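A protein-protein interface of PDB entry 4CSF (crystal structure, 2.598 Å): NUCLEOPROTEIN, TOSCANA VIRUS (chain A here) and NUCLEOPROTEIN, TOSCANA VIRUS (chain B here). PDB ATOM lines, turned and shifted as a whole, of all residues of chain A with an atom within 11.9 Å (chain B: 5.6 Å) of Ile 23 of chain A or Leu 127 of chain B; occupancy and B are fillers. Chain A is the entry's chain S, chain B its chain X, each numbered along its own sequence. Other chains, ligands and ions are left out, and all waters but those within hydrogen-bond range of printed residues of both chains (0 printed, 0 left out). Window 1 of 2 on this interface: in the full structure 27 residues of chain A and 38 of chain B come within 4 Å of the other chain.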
ATOM      1  N   PHE A  13      -0.788  27.704 -14.603  1.00  0.00           N
ATOM      2  CA  PHE A  13       0.222  27.696 -13.550  1.00  0.00           C
ATOM      3  C   PHE A  13      -0.384  27.407 -12.185  1.00  0.00           C
ATOM      4  O   PHE A  13       0.339  27.169 -11.218  1.00  0.00           O
ATOM      5  CB  PHE A  13       1.003  29.011 -13.531  1.00  0.00           C
ATOM      6  CG  PHE A  13       2.202  29.006 -14.429  1.00  0.00           C
ATOM      7  CD1 PHE A  13       2.063  29.215 -15.792  1.00  0.00           C
ATOM      8  CD2 PHE A  13       3.468  28.774 -13.912  1.00  0.00           C
ATOM      9  CE1 PHE A  13       3.169  29.204 -16.625  1.00  0.00           C
ATOM     10  CE2 PHE A  13       4.581  28.762 -14.740  1.00  0.00           C
ATOM     11  CZ  PHE A  13       4.429  28.978 -16.099  1.00  0.00           C
ATOM     12  N   LEU A  14      -1.712  27.436 -12.113  1.00  0.00           N
ATOM     13  CA  LEU A  14      -2.432  27.031 -10.917  1.00  0.00           C
ATOM     14  C   LEU A  14      -2.119  25.572 -10.620  1.00  0.00           C
ATOM     15  O   LEU A  14      -1.903  25.186  -9.471  1.00  0.00           O
ATOM     16  CB  LEU A  14      -3.937  27.178 -11.142  1.00  0.00           C
ATOM     17  CG  LEU A  14      -4.845  27.560  -9.961  1.00  0.00           C
ATOM     18  CD1 LEU A  14      -6.238  26.908 -10.033  1.00  0.00           C
ATOM     19  CD2 LEU A  14      -4.191  27.395  -8.578  1.00  0.00           C
ATOM     20  N   ASP A  15      -2.097  24.764 -11.674  1.00  0.00           N
ATOM     21  CA  ASP A  15      -1.865  23.331 -11.536  1.00  0.00           C
ATOM     22  C   ASP A  15      -0.393  22.977 -11.739  1.00  0.00           C
ATOM     23  O   ASP A  15      -0.025  21.802 -11.741  1.00  0.00           O
ATOM     24  CB  ASP A  15      -2.742  22.556 -12.523  1.00  0.00           C
ATOM     25  CG  ASP A  15      -4.223  22.856 -12.348  1.00  0.00           C
ATOM     26  OD1 ASP A  15      -4.677  22.961 -11.187  1.00  0.00           O
ATOM     27  OD2 ASP A  15      -4.933  22.990 -13.369  1.00  0.00           O
ATOM     28  N   GLU A  16       0.444  23.995 -11.909  1.00  0.00           N
ATOM     29  CA  GLU A  16       1.874  23.771 -12.069  1.00  0.00           C
ATOM     30  C   GLU A  16       2.508  23.521 -10.698  1.00  0.00           C
ATOM     31  O   GLU A  16       2.050  24.063  -9.687  1.00  0.00           O
ATOM     32  CB  GLU A  16       2.524  24.958 -12.779  1.00  0.00           C
ATOM     33  CG  GLU A  16       3.865  24.640 -13.416  1.00  0.00           C
ATOM     34  CD  GLU A  16       3.752  24.002 -14.785  1.00  0.00           C
ATOM     35  OE1 GLU A  16       2.889  24.435 -15.576  1.00  0.00           O
ATOM     36  OE2 GLU A  16       4.541  23.079 -15.080  1.00  0.00           O
ATOM     37  N   SER A  17       3.551  22.693 -10.669  1.00  0.00           N
ATOM     38  CA  SER A  17       4.152  22.233  -9.412  1.00  0.00           C
ATOM     39  C   SER A  17       4.795  23.339  -8.573  1.00  0.00           C
ATOM     40  O   SER A  17       5.602  24.129  -9.066  1.00  0.00           O
ATOM     41  CB  SER A  17       5.178  21.127  -9.680  1.00  0.00           C
ATOM     42  OG  SER A  17       6.279  21.616 -10.432  1.00  0.00           O
ATOM     43  N   ALA A  18       4.422  23.379  -7.299  1.00  0.00           N
ATOM     44  CA  ALA A  18       5.014  24.307  -6.343  1.00  0.00           C
ATOM     45  C   ALA A  18       5.707  23.512  -5.236  1.00  0.00           C
ATOM     46  O   ALA A  18       5.298  23.559  -4.073  1.00  0.00           O
ATOM     47  CB  ALA A  18       3.951  25.221  -5.758  1.00  0.00           C
ATOM     48  N   ASP A  19       6.755  22.784  -5.617  1.00  0.00           N
ATOM     49  CA  ASP A  19       7.480  21.893  -4.716  1.00  0.00           C
ATOM     50  C   ASP A  19       8.192  22.635  -3.579  1.00  0.00           C
ATOM     51  O   ASP A  19       9.074  23.459  -3.830  1.00  0.00           O
ATOM     52  CB  ASP A  19       8.499  21.084  -5.513  1.00  0.00           C
ATOM     53  CG  ASP A  19       8.963  19.856  -4.774  1.00  0.00           C
ATOM     54  OD1 ASP A  19       8.232  18.853  -4.841  1.00  0.00           O
ATOM     55  OD2 ASP A  19      10.047  19.888  -4.145  1.00  0.00           O
ATOM     56  N   SER A  20       7.816  22.333  -2.337  1.00  0.00           N
ATOM     57  CA  SER A  20       8.436  22.948  -1.163  1.00  0.00           C
ATOM     58  C   SER A  20       9.967  22.850  -1.154  1.00  0.00           C
ATOM     59  O   SER A  20      10.664  23.841  -0.893  1.00  0.00           O
ATOM     60  CB  SER A  20       7.859  22.342   0.119  1.00  0.00           C
ATOM     61  OG  SER A  20       8.782  22.445   1.197  1.00  0.00           O
ATOM     62  N   GLY A  21      10.481  21.660  -1.456  1.00  0.00           N
ATOM     63  CA  GLY A  21      11.914  21.415  -1.444  1.00  0.00           C
ATOM     64  C   GLY A  21      12.708  22.263  -2.423  1.00  0.00           C
ATOM     65  O   GLY A  21      13.691  22.905  -2.044  1.00  0.00           O
ATOM     66  N   THR A  22      12.283  22.272  -3.683  1.00  0.00           N
ATOM     67  CA  THR A  22      12.974  23.035  -4.715  1.00  0.00           C
ATOM     68  C   THR A  22      12.839  24.544  -4.487  1.00  0.00           C
ATOM     69  O   THR A  22      13.788  25.297  -4.703  1.00  0.00           O
ATOM     70  CB  THR A  22      12.487  22.660  -6.142  1.00  0.00           C
ATOM     71  OG1 THR A  22      11.173  23.182  -6.367  1.00  0.00           O
ATOM     72  CG2 THR A  22      12.469  21.149  -6.328  1.00  0.00           C
ATOM     73  N   ILE A  23      11.662  24.978  -4.043  1.00  0.00           N
ATOM     74  CA  ILE A  23      11.430  26.388  -3.744  1.00  0.00           C
ATOM     75  C   ILE A  23      12.359  26.897  -2.636  1.00  0.00           C
ATOM     76  O   ILE A  23      12.960  27.967  -2.765  1.00  0.00           O
ATOM     77  CB  ILE A  23       9.954  26.659  -3.364  1.00  0.00           C
ATOM     78  CG1 ILE A  23       9.058  26.571  -4.602  1.00  0.00           C
ATOM     79  CG2 ILE A  23       9.797  28.027  -2.707  1.00  0.00           C
ATOM     80  CD1 ILE A  23       7.570  26.727  -4.310  1.00  0.00           C
ATOM     81  N   ASN A  24      12.482  26.123  -1.558  1.00  0.00           N
ATOM     82  CA  ASN A  24      13.351  26.500  -0.445  1.00  0.00           C
ATOM     83  C   ASN A  24      14.828  26.526  -0.835  1.00  0.00           C
ATOM     84  O   ASN A  24      15.610  27.316  -0.298  1.00  0.00           O
ATOM     85  CB  ASN A  24      13.115  25.599   0.775  1.00  0.00           C
ATOM     86  CG  ASN A  24      11.925  26.053   1.625  1.00  0.00           C
ATOM     87  OD1 ASN A  24      11.710  27.252   1.837  1.00  0.00           O
ATOM     88  ND2 ASN A  24      11.151  25.091   2.116  1.00  0.00           N
ATOM     89  N   ALA A  25      15.204  25.673  -1.781  1.00  0.00           N
ATOM     90  CA  ALA A  25      16.566  25.671  -2.303  1.00  0.00           C
ATOM     91  C   ALA A  25      16.859  26.947  -3.100  1.00  0.00           C
ATOM     92  O   ALA A  25      17.956  27.502  -3.010  1.00  0.00           O
ATOM     93  CB  ALA A  25      16.808  24.435  -3.154  1.00  0.00           C
ATOM     94  N   TRP A  26      15.875  27.402  -3.875  1.00  0.00           N
ATOM     95  CA  TRP A  26      15.988  28.659  -4.614  1.00  0.00           C
ATOM     96  C   TRP A  26      16.106  29.829  -3.649  1.00  0.00           C
ATOM     97  O   TRP A  26      16.944  30.715  -3.838  1.00  0.00           O
ATOM     98  CB  TRP A  26      14.782  28.864  -5.537  1.00  0.00           C
ATOM     99  CG  TRP A  26      14.749  27.914  -6.700  1.00  0.00           C
ATOM    100  CD1 TRP A  26      15.800  27.229  -7.227  1.00  0.00           C
ATOM    101  CD2 TRP A  26      13.595  27.537  -7.466  1.00  0.00           C
ATOM    102  NE1 TRP A  26      15.373  26.448  -8.278  1.00  0.00           N
ATOM    103  CE2 TRP A  26      14.030  26.619  -8.442  1.00  0.00           C
ATOM    104  CE3 TRP A  26      12.245  27.884  -7.420  1.00  0.00           C
ATOM    105  CZ2 TRP A  26      13.150  26.050  -9.369  1.00  0.00           C
ATOM    106  CZ3 TRP A  26      11.377  27.317  -8.343  1.00  0.00           C
ATOM    107  CH2 TRP A  26      11.834  26.414  -9.303  1.00  0.00           C
ATOM    108  N   VAL A  27      15.261  29.822  -2.620  1.00  0.00           N
ATOM    109  CA  VAL A  27      15.287  30.850  -1.584  1.00  0.00           C
ATOM    110  C   VAL A  27      16.685  30.973  -0.992  1.00  0.00           C
ATOM    111  O   VAL A  27      17.207  32.083  -0.846  1.00  0.00           O
ATOM    112  CB  VAL A  27      14.274  30.550  -0.456  1.00  0.00           C
ATOM    113  CG1 VAL A  27      14.464  31.513   0.704  1.00  0.00           C
ATOM    114  CG2 VAL A  27      12.843  30.626  -0.989  1.00  0.00           C
ATOM    115  N   ASN A  28      17.290  29.827  -0.683  1.00  0.00           N
ATOM    116  CA  ASN A  28      18.640  29.782  -0.123  1.00  0.00           C
ATOM    117  C   ASN A  28      19.711  30.340  -1.068  1.00  0.00           C
ATOM    118  O   ASN A  28      20.675  30.963  -0.619  1.00  0.00           O
ATOM    119  CB  ASN A  28      18.995  28.360   0.324  1.00  0.00           C
ATOM    120  CG  ASN A  28      18.194  27.908   1.538  1.00  0.00           C
ATOM    121  OD1 ASN A  28      17.376  28.657   2.075  1.00  0.00           O
ATOM    122  ND2 ASN A  28      18.420  26.676   1.970  1.00  0.00           N
ATOM    123  N   GLU A  29      19.541  30.118  -2.371  1.00  0.00           N
ATOM    124  CA  GLU A  29      20.466  30.649  -3.371  1.00  0.00           C
ATOM    125  C   GLU A  29      20.304  32.157  -3.530  1.00  0.00           C
ATOM    126  O   GLU A  29      21.283  32.895  -3.651  1.00  0.00           O
ATOM    127  CB  GLU A  29      20.224  29.983  -4.728  1.00  0.00           C
ATOM    128  CG  GLU A  29      20.611  28.514  -4.798  1.00  0.00           C
ATOM    129  CD  GLU A  29      20.146  27.859  -6.086  1.00  0.00           C
ATOM    130  OE1 GLU A  29      19.263  28.436  -6.759  1.00  0.00           O
ATOM    131  OE2 GLU A  29      20.659  26.769  -6.423  1.00  0.00           O
ATOM    132  N   PHE A  30      19.051  32.602  -3.531  1.00  0.00           N
ATOM    133  CA  PHE A  30      18.709  33.984  -3.839  1.00  0.00           C
ATOM    134  C   PHE A  30      18.758  34.910  -2.634  1.00  0.00           C
ATOM    135  O   PHE A  30      18.789  36.133  -2.793  1.00  0.00           O
ATOM    136  CB  PHE A  30      17.308  34.042  -4.444  1.00  0.00           C
ATOM    137  CG  PHE A  30      17.203  33.391  -5.789  1.00  0.00           C
ATOM    138  CD1 PHE A  30      18.304  33.326  -6.631  1.00  0.00           C
ATOM    139  CD2 PHE A  30      15.999  32.851  -6.218  1.00  0.00           C
ATOM    140  CE1 PHE A  30      18.207  32.729  -7.885  1.00  0.00           C
ATOM    141  CE2 PHE A  30      15.894  32.249  -7.468  1.00  0.00           C
ATOM    142  CZ  PHE A  30      16.997  32.191  -8.301  1.00  0.00           C
ATOM    143  N   ALA A  31      18.748  34.334  -1.436  1.00  0.00           N
ATOM    144  CA  ALA A  31      18.658  35.121  -0.205  1.00  0.00           C
ATOM    145  C   ALA A  31      19.754  36.172  -0.087  1.00  0.00           C
ATOM    146  O   ALA A  31      20.830  36.034  -0.673  1.00  0.00           O
ATOM    147  CB  ALA A  31      18.681  34.210   1.011  1.00  0.00           C
ATOM    148  N   TYR A  32      19.464  37.231   0.663  1.00  0.00           N
ATOM    149  CA  TYR A  32      20.453  38.271   0.929  1.00  0.00           C
ATOM    150  C   TYR A  32      21.708  37.672   1.550  1.00  0.00           C
ATOM    151  O   TYR A  32      21.627  36.837   2.455  1.00  0.00           O
ATOM    152  CB  TYR A  32      19.872  39.347   1.850  1.00  0.00           C
ATOM    153  CG  TYR A  32      20.906  40.312   2.379  1.00  0.00           C
ATOM    154  CD1 TYR A  32      21.349  41.382   1.609  1.00  0.00           C
ATOM    155  CD2 TYR A  32      21.443  40.155   3.650  1.00  0.00           C
ATOM    156  CE1 TYR A  32      22.299  42.269   2.094  1.00  0.00           C
ATOM    157  CE2 TYR A  32      22.396  41.033   4.144  1.00  0.00           C
ATOM    158  CZ  TYR A  32      22.818  42.088   3.364  1.00  0.00           C
ATOM    159  OH  TYR A  32      23.763  42.961   3.857  1.00  0.00           O
ATOM    160  N   ARG A 213      16.840  38.807  11.746  1.00  0.00           N
ATOM    161  CA  ARG A 213      16.321  37.590  12.353  1.00  0.00           C
ATOM    162  C   ARG A 213      17.378  36.847  13.170  1.00  0.00           C
ATOM    163  O   ARG A 213      17.175  35.692  13.545  1.00  0.00           O
ATOM    164  CB  ARG A 213      15.750  36.679  11.268  1.00  0.00           C
ATOM    165  CG  ARG A 213      14.976  37.420  10.191  1.00  0.00           C
ATOM    166  CD  ARG A 213      13.529  36.960  10.114  1.00  0.00           C
ATOM    167  NE  ARG A 213      13.034  36.970   8.740  1.00  0.00           N
ATOM    168  CZ  ARG A 213      12.301  37.943   8.207  1.00  0.00           C
ATOM    169  NH1 ARG A 213      11.956  39.000   8.932  1.00  0.00           N
ATOM    170  NH2 ARG A 213      11.904  37.852   6.944  1.00  0.00           N
ATOM    171  N   VAL B  64       9.867  33.428  -7.253  1.00  0.00           N
ATOM    172  CA  VAL B  64      10.498  33.258  -5.945  1.00  0.00           C
ATOM    173  C   VAL B  64      11.555  34.339  -5.708  1.00  0.00           C
ATOM    174  O   VAL B  64      11.610  34.944  -4.634  1.00  0.00           O
ATOM    175  CB  VAL B  64      11.131  31.864  -5.811  1.00  0.00           C
ATOM    176  CG1 VAL B  64      12.041  31.799  -4.590  1.00  0.00           C
ATOM    177  CG2 VAL B  64      10.041  30.793  -5.747  1.00  0.00           C
ATOM    178  N   LEU B  67       9.761  37.483  -4.911  1.00  0.00           N
ATOM    179  CA  LEU B  67       9.159  37.466  -3.582  1.00  0.00           C
ATOM    180  C   LEU B  67      10.165  37.750  -2.463  1.00  0.00           C
ATOM    181  O   LEU B  67       9.835  38.434  -1.489  1.00  0.00           O
ATOM    182  CB  LEU B  67       8.448  36.134  -3.321  1.00  0.00           C
ATOM    183  CG  LEU B  67       7.261  35.799  -4.228  1.00  0.00           C
ATOM    184  CD1 LEU B  67       6.609  34.488  -3.821  1.00  0.00           C
ATOM    185  CD2 LEU B  67       6.247  36.922  -4.220  1.00  0.00           C
ATOM    186  N   VAL B  68      11.388  37.243  -2.604  1.00  0.00           N
ATOM    187  CA  VAL B  68      12.372  37.368  -1.527  1.00  0.00           C
ATOM    188  C   VAL B  68      13.385  38.506  -1.698  1.00  0.00           C
ATOM    189  O   VAL B  68      13.995  38.933  -0.721  1.00  0.00           O
ATOM    190  CB  VAL B  68      13.128  36.029  -1.262  1.00  0.00           C
ATOM    191  CG1 VAL B  68      12.180  34.843  -1.365  1.00  0.00           C
ATOM    192  CG2 VAL B  68      14.297  35.866  -2.203  1.00  0.00           C
ATOM    193  N   TRP B 119       0.479  30.926  -9.860  1.00  0.00           N
ATOM    194  CA  TRP B 119       1.568  30.192  -9.219  1.00  0.00           C
ATOM    195  C   TRP B 119       2.147  30.963  -8.030  1.00  0.00           C
ATOM    196  O   TRP B 119       2.467  30.370  -6.992  1.00  0.00           O
ATOM    197  CB  TRP B 119       2.674  29.827 -10.213  1.00  0.00           C
ATOM    198  CG  TRP B 119       3.633  28.807  -9.645  1.00  0.00           C
ATOM    199  CD1 TRP B 119       3.501  27.447  -9.683  1.00  0.00           C
ATOM    200  CD2 TRP B 119       4.854  29.071  -8.933  1.00  0.00           C
ATOM    201  NE1 TRP B 119       4.567  26.851  -9.049  1.00  0.00           N
ATOM    202  CE2 TRP B 119       5.413  27.825  -8.581  1.00  0.00           C
ATOM    203  CE3 TRP B 119       5.529  30.238  -8.568  1.00  0.00           C
ATOM    204  CZ2 TRP B 119       6.617  27.714  -7.875  1.00  0.00           C
ATOM    205  CZ3 TRP B 119       6.723  30.127  -7.869  1.00  0.00           C
ATOM    206  CH2 TRP B 119       7.254  28.875  -7.529  1.00  0.00           C
ATOM    207  N   ALA B 123       3.195  29.783  -4.138  1.00  0.00           N
ATOM    208  CA  ALA B 123       4.538  29.876  -3.579  1.00  0.00           C
ATOM    209  C   ALA B 123       4.509  30.580  -2.225  1.00  0.00           C
ATOM    210  O   ALA B 123       5.247  30.216  -1.309  1.00  0.00           O
ATOM    211  CB  ALA B 123       5.462  30.608  -4.544  1.00  0.00           C
ATOM    212  N   LEU B 124       3.645  31.587  -2.110  1.00  0.00           N
ATOM    213  CA  LEU B 124       3.478  32.337  -0.867  1.00  0.00           C
ATOM    214  C   LEU B 124       3.116  31.427   0.303  1.00  0.00           C
ATOM    215  O   LEU B 124       3.487  31.694   1.443  1.00  0.00           O
ATOM    216  CB  LEU B 124       2.408  33.423  -1.036  1.00  0.00           C
ATOM    217  CG  LEU B 124       2.792  34.629  -1.889  1.00  0.00           C
ATOM    218  CD1 LEU B 124       1.598  35.550  -2.110  1.00  0.00           C
ATOM    219  CD2 LEU B 124       3.949  35.387  -1.238  1.00  0.00           C
ATOM    220  N   ARG B 125       2.398  30.350   0.010  1.00  0.00           N
ATOM    221  CA  ARG B 125       1.983  29.386   1.026  1.00  0.00           C
ATOM    222  C   ARG B 125       3.188  28.643   1.612  1.00  0.00           C
ATOM    223  O   ARG B 125       3.107  28.066   2.702  1.00  0.00           O
ATOM    224  CB  ARG B 125       0.984  28.396   0.413  1.00  0.00           C
ATOM    225  CG  ARG B 125       0.284  27.470   1.401  1.00  0.00           C
ATOM    226  CD  ARG B 125      -0.473  26.349   0.679  1.00  0.00           C
ATOM    227  NE  ARG B 125       0.415  25.521  -0.139  1.00  0.00           N
ATOM    228  CZ  ARG B 125       0.475  25.564  -1.468  1.00  0.00           C
ATOM    229  NH1 ARG B 125      -0.313  26.390  -2.146  1.00  0.00           N
ATOM    230  NH2 ARG B 125       1.318  24.775  -2.123  1.00  0.00           N
ATOM    231  N   VAL B 126       4.309  28.690   0.894  1.00  0.00           N
ATOM    232  CA  VAL B 126       5.509  27.933   1.248  1.00  0.00           C
ATOM    233  C   VAL B 126       6.613  28.770   1.910  1.00  0.00           C
ATOM    234  O   VAL B 126       7.200  28.354   2.912  1.00  0.00           O
ATOM    235  CB  VAL B 126       6.088  27.208  -0.002  1.00  0.00           C
ATOM    236  CG1 VAL B 126       7.427  26.552   0.313  1.00  0.00           C
ATOM    237  CG2 VAL B 126       5.100  26.181  -0.531  1.00  0.00           C
ATOM    238  N   LEU B 127       6.887  29.946   1.353  1.00  0.00           N
ATOM    239  CA  LEU B 127       8.020  30.759   1.795  1.00  0.00           C
ATOM    240  C   LEU B 127       7.642  32.015   2.589  1.00  0.00           C
ATOM    241  O   LEU B 127       8.377  33.005   2.568  1.00  0.00           O
ATOM    242  CB  LEU B 127       8.899  31.139   0.591  1.00  0.00           C
ATOM    243  CG  LEU B 127       8.199  31.540  -0.714  1.00  0.00           C
ATOM    244  CD1 LEU B 127       7.332  32.781  -0.550  1.00  0.00           C
ATOM    245  CD2 LEU B 127       9.211  31.747  -1.828  1.00  0.00           C
ATOM    246  N   SER B 128       6.515  31.972   3.295  1.00  0.00           N
ATOM    247  CA  SER B 128       5.994  33.164   3.971  1.00  0.00           C
ATOM    248  C   SER B 128       6.915  33.745   5.043  1.00  0.00           C
ATOM    249  O   SER B 128       6.793  34.922   5.384  1.00  0.00           O
ATOM    250  CB  SER B 128       4.601  32.902   4.555  1.00  0.00           C
ATOM    251  OG  SER B 128       4.634  31.874   5.533  1.00  0.00           O
ATOM    252  N   GLU B 129       7.833  32.931   5.566  1.00  0.00           N
ATOM    253  CA  GLU B 129       8.766  33.398   6.591  1.00  0.00           C
ATOM    254  C   GLU B 129      10.045  34.007   6.016  1.00  0.00           C
ATOM    255  O   GLU B 129      10.870  34.544   6.761  1.00  0.00           O
ATOM    256  CB  GLU B 129       9.108  32.283   7.580  1.00  0.00           C
ATOM    257  CG  GLU B 129       7.977  31.920   8.523  1.00  0.00           C
ATOM    258  CD  GLU B 129       7.471  33.112   9.317  1.00  0.00           C
ATOM    259  OE1 GLU B 129       8.232  33.640  10.159  1.00  0.00           O
ATOM    260  OE2 GLU B 129       6.310  33.520   9.095  1.00  0.00           O
ATOM    261  N   SER B 130      10.200  33.930   4.693  1.00  0.00           N
ATOM    262  CA  SER B 130      11.363  34.503   4.015  1.00  0.00           C
ATOM    263  C   SER B 130      11.032  35.822   3.308  1.00  0.00           C
ATOM    264  O   SER B 130      11.885  36.402   2.626  1.00  0.00           O
ATOM    265  CB  SER B 130      11.951  33.504   3.016  1.00  0.00           C
ATOM    266  OG  SER B 130      12.306  32.285   3.653  1.00  0.00           O
ATOM    267  N   LEU B 131       9.797  36.291   3.483  1.00  0.00           N
ATOM    268  CA  LEU B 131       9.341  37.552   2.892  1.00  0.00           C
ATOM    269  C   LEU B 131       9.823  38.744   3.717  1.00  0.00           C
ATOM    270  O   LEU B 131      10.153  38.583   4.893  1.00  0.00           O
ATOM    271  CB  LEU B 131       7.811  37.563   2.791  1.00  0.00           C
ATOM    272  CG  LEU B 131       7.208  36.485   1.894  1.00  0.00           C
ATOM    273  CD1 LEU B 131       5.697  36.404   2.063  1.00  0.00           C
ATOM    274  CD2 LEU B 131       7.586  36.745   0.439  1.00  0.00           C
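O of Ser 17 of chain A lies within hydrogen-bond range of NE1 of Trp 119 of chain B.
The guanidinium group (NH2) of Arg 213 of chain A lies within hydrogen-bond range of the backbone carbonyl oxygen (O) of Glu 129 of chain B.
The backbone carbonyl oxygen of Leu 131 of chain B is in hydrogen-bond range of the guanidinium group of Arg 213 of chain A (2.8 Å).
Among the printed residues, merely in contact across the chains: Phe 13 of chain A with Trp 119 of chain B (3.5 Å), Glu 16 of chain A with Trp 119 of chain B (3.7 Å), Ala 18 of chain A with Trp 119 of chain B (3.7 Å), Ile 23 of chain A with Trp 119 of chain B (3.8 Å), Ile 23 of chain A with Leu 127 of chain B (3.9 Å), Val 27 of chain A with Val 64 of chain B (3.9 Å), Val 27 of chain A with Leu 127 of chain B (3.9 Å) and Val 27 of chain A with Ser 130 of chain B (3.7 Å).
Of chain B, only Trp 119 and Leu 127 come within 4 Å of Ile 23 of chain A.
Of the printed residues of chain A, Leu 127 of chain B touches Ile 23 (3.9 Å) and Val 27 (3.9 Å).
No residue of chain A comes within 4 Å of Leu 67 of chain B.
No residue of chain A comes within 4 Å of Ala 123 of chain B.
No residue of chain A comes within 4 Å of Leu 124 of chain B.
No residue of chain A comes within 4 Å of Val 126 of chain B.
No residue of chain A comes within 4 Å of Ser 128 of chain B.
Ser 130 of chain B touches just one residue of chain A: Val 27.
Printed residues of chain B within 4 Å of Ala 18 of chain A: Trp 119.
Of the printed residues of chain B, Glu 16 of chain A touches Trp 119 (3.7 Å).
Printed residues of chain A within 4 Å of Val 64 of chain B: Val 27.
Of the printed residues of chain B, Ser 17 of chain A touches Trp 119.
Asp 15 of chain A touches none of the printed residues of chain B.
The nearest printed residue of chain B that does not touch Ile 23 of chain A is Val 126 of chain B (4.1 Å).
The nearest printed residue of chain A that does not touch Trp 119 of chain B is Trp 26 of chain A (4.5 Å).
Hydrophobic or aromatic side chains of chain A within 4 Å of the printed part of chain B: Phe 13, Ala 18, Ile 23 and Val 27.
Of the 13 printed residues of chain B, 6 touch a printed residue of chain A.
Hydrophobic or aromatic side chains of chain B that line the printed part of chain A: Val 64, Trp 119 and Leu 127.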
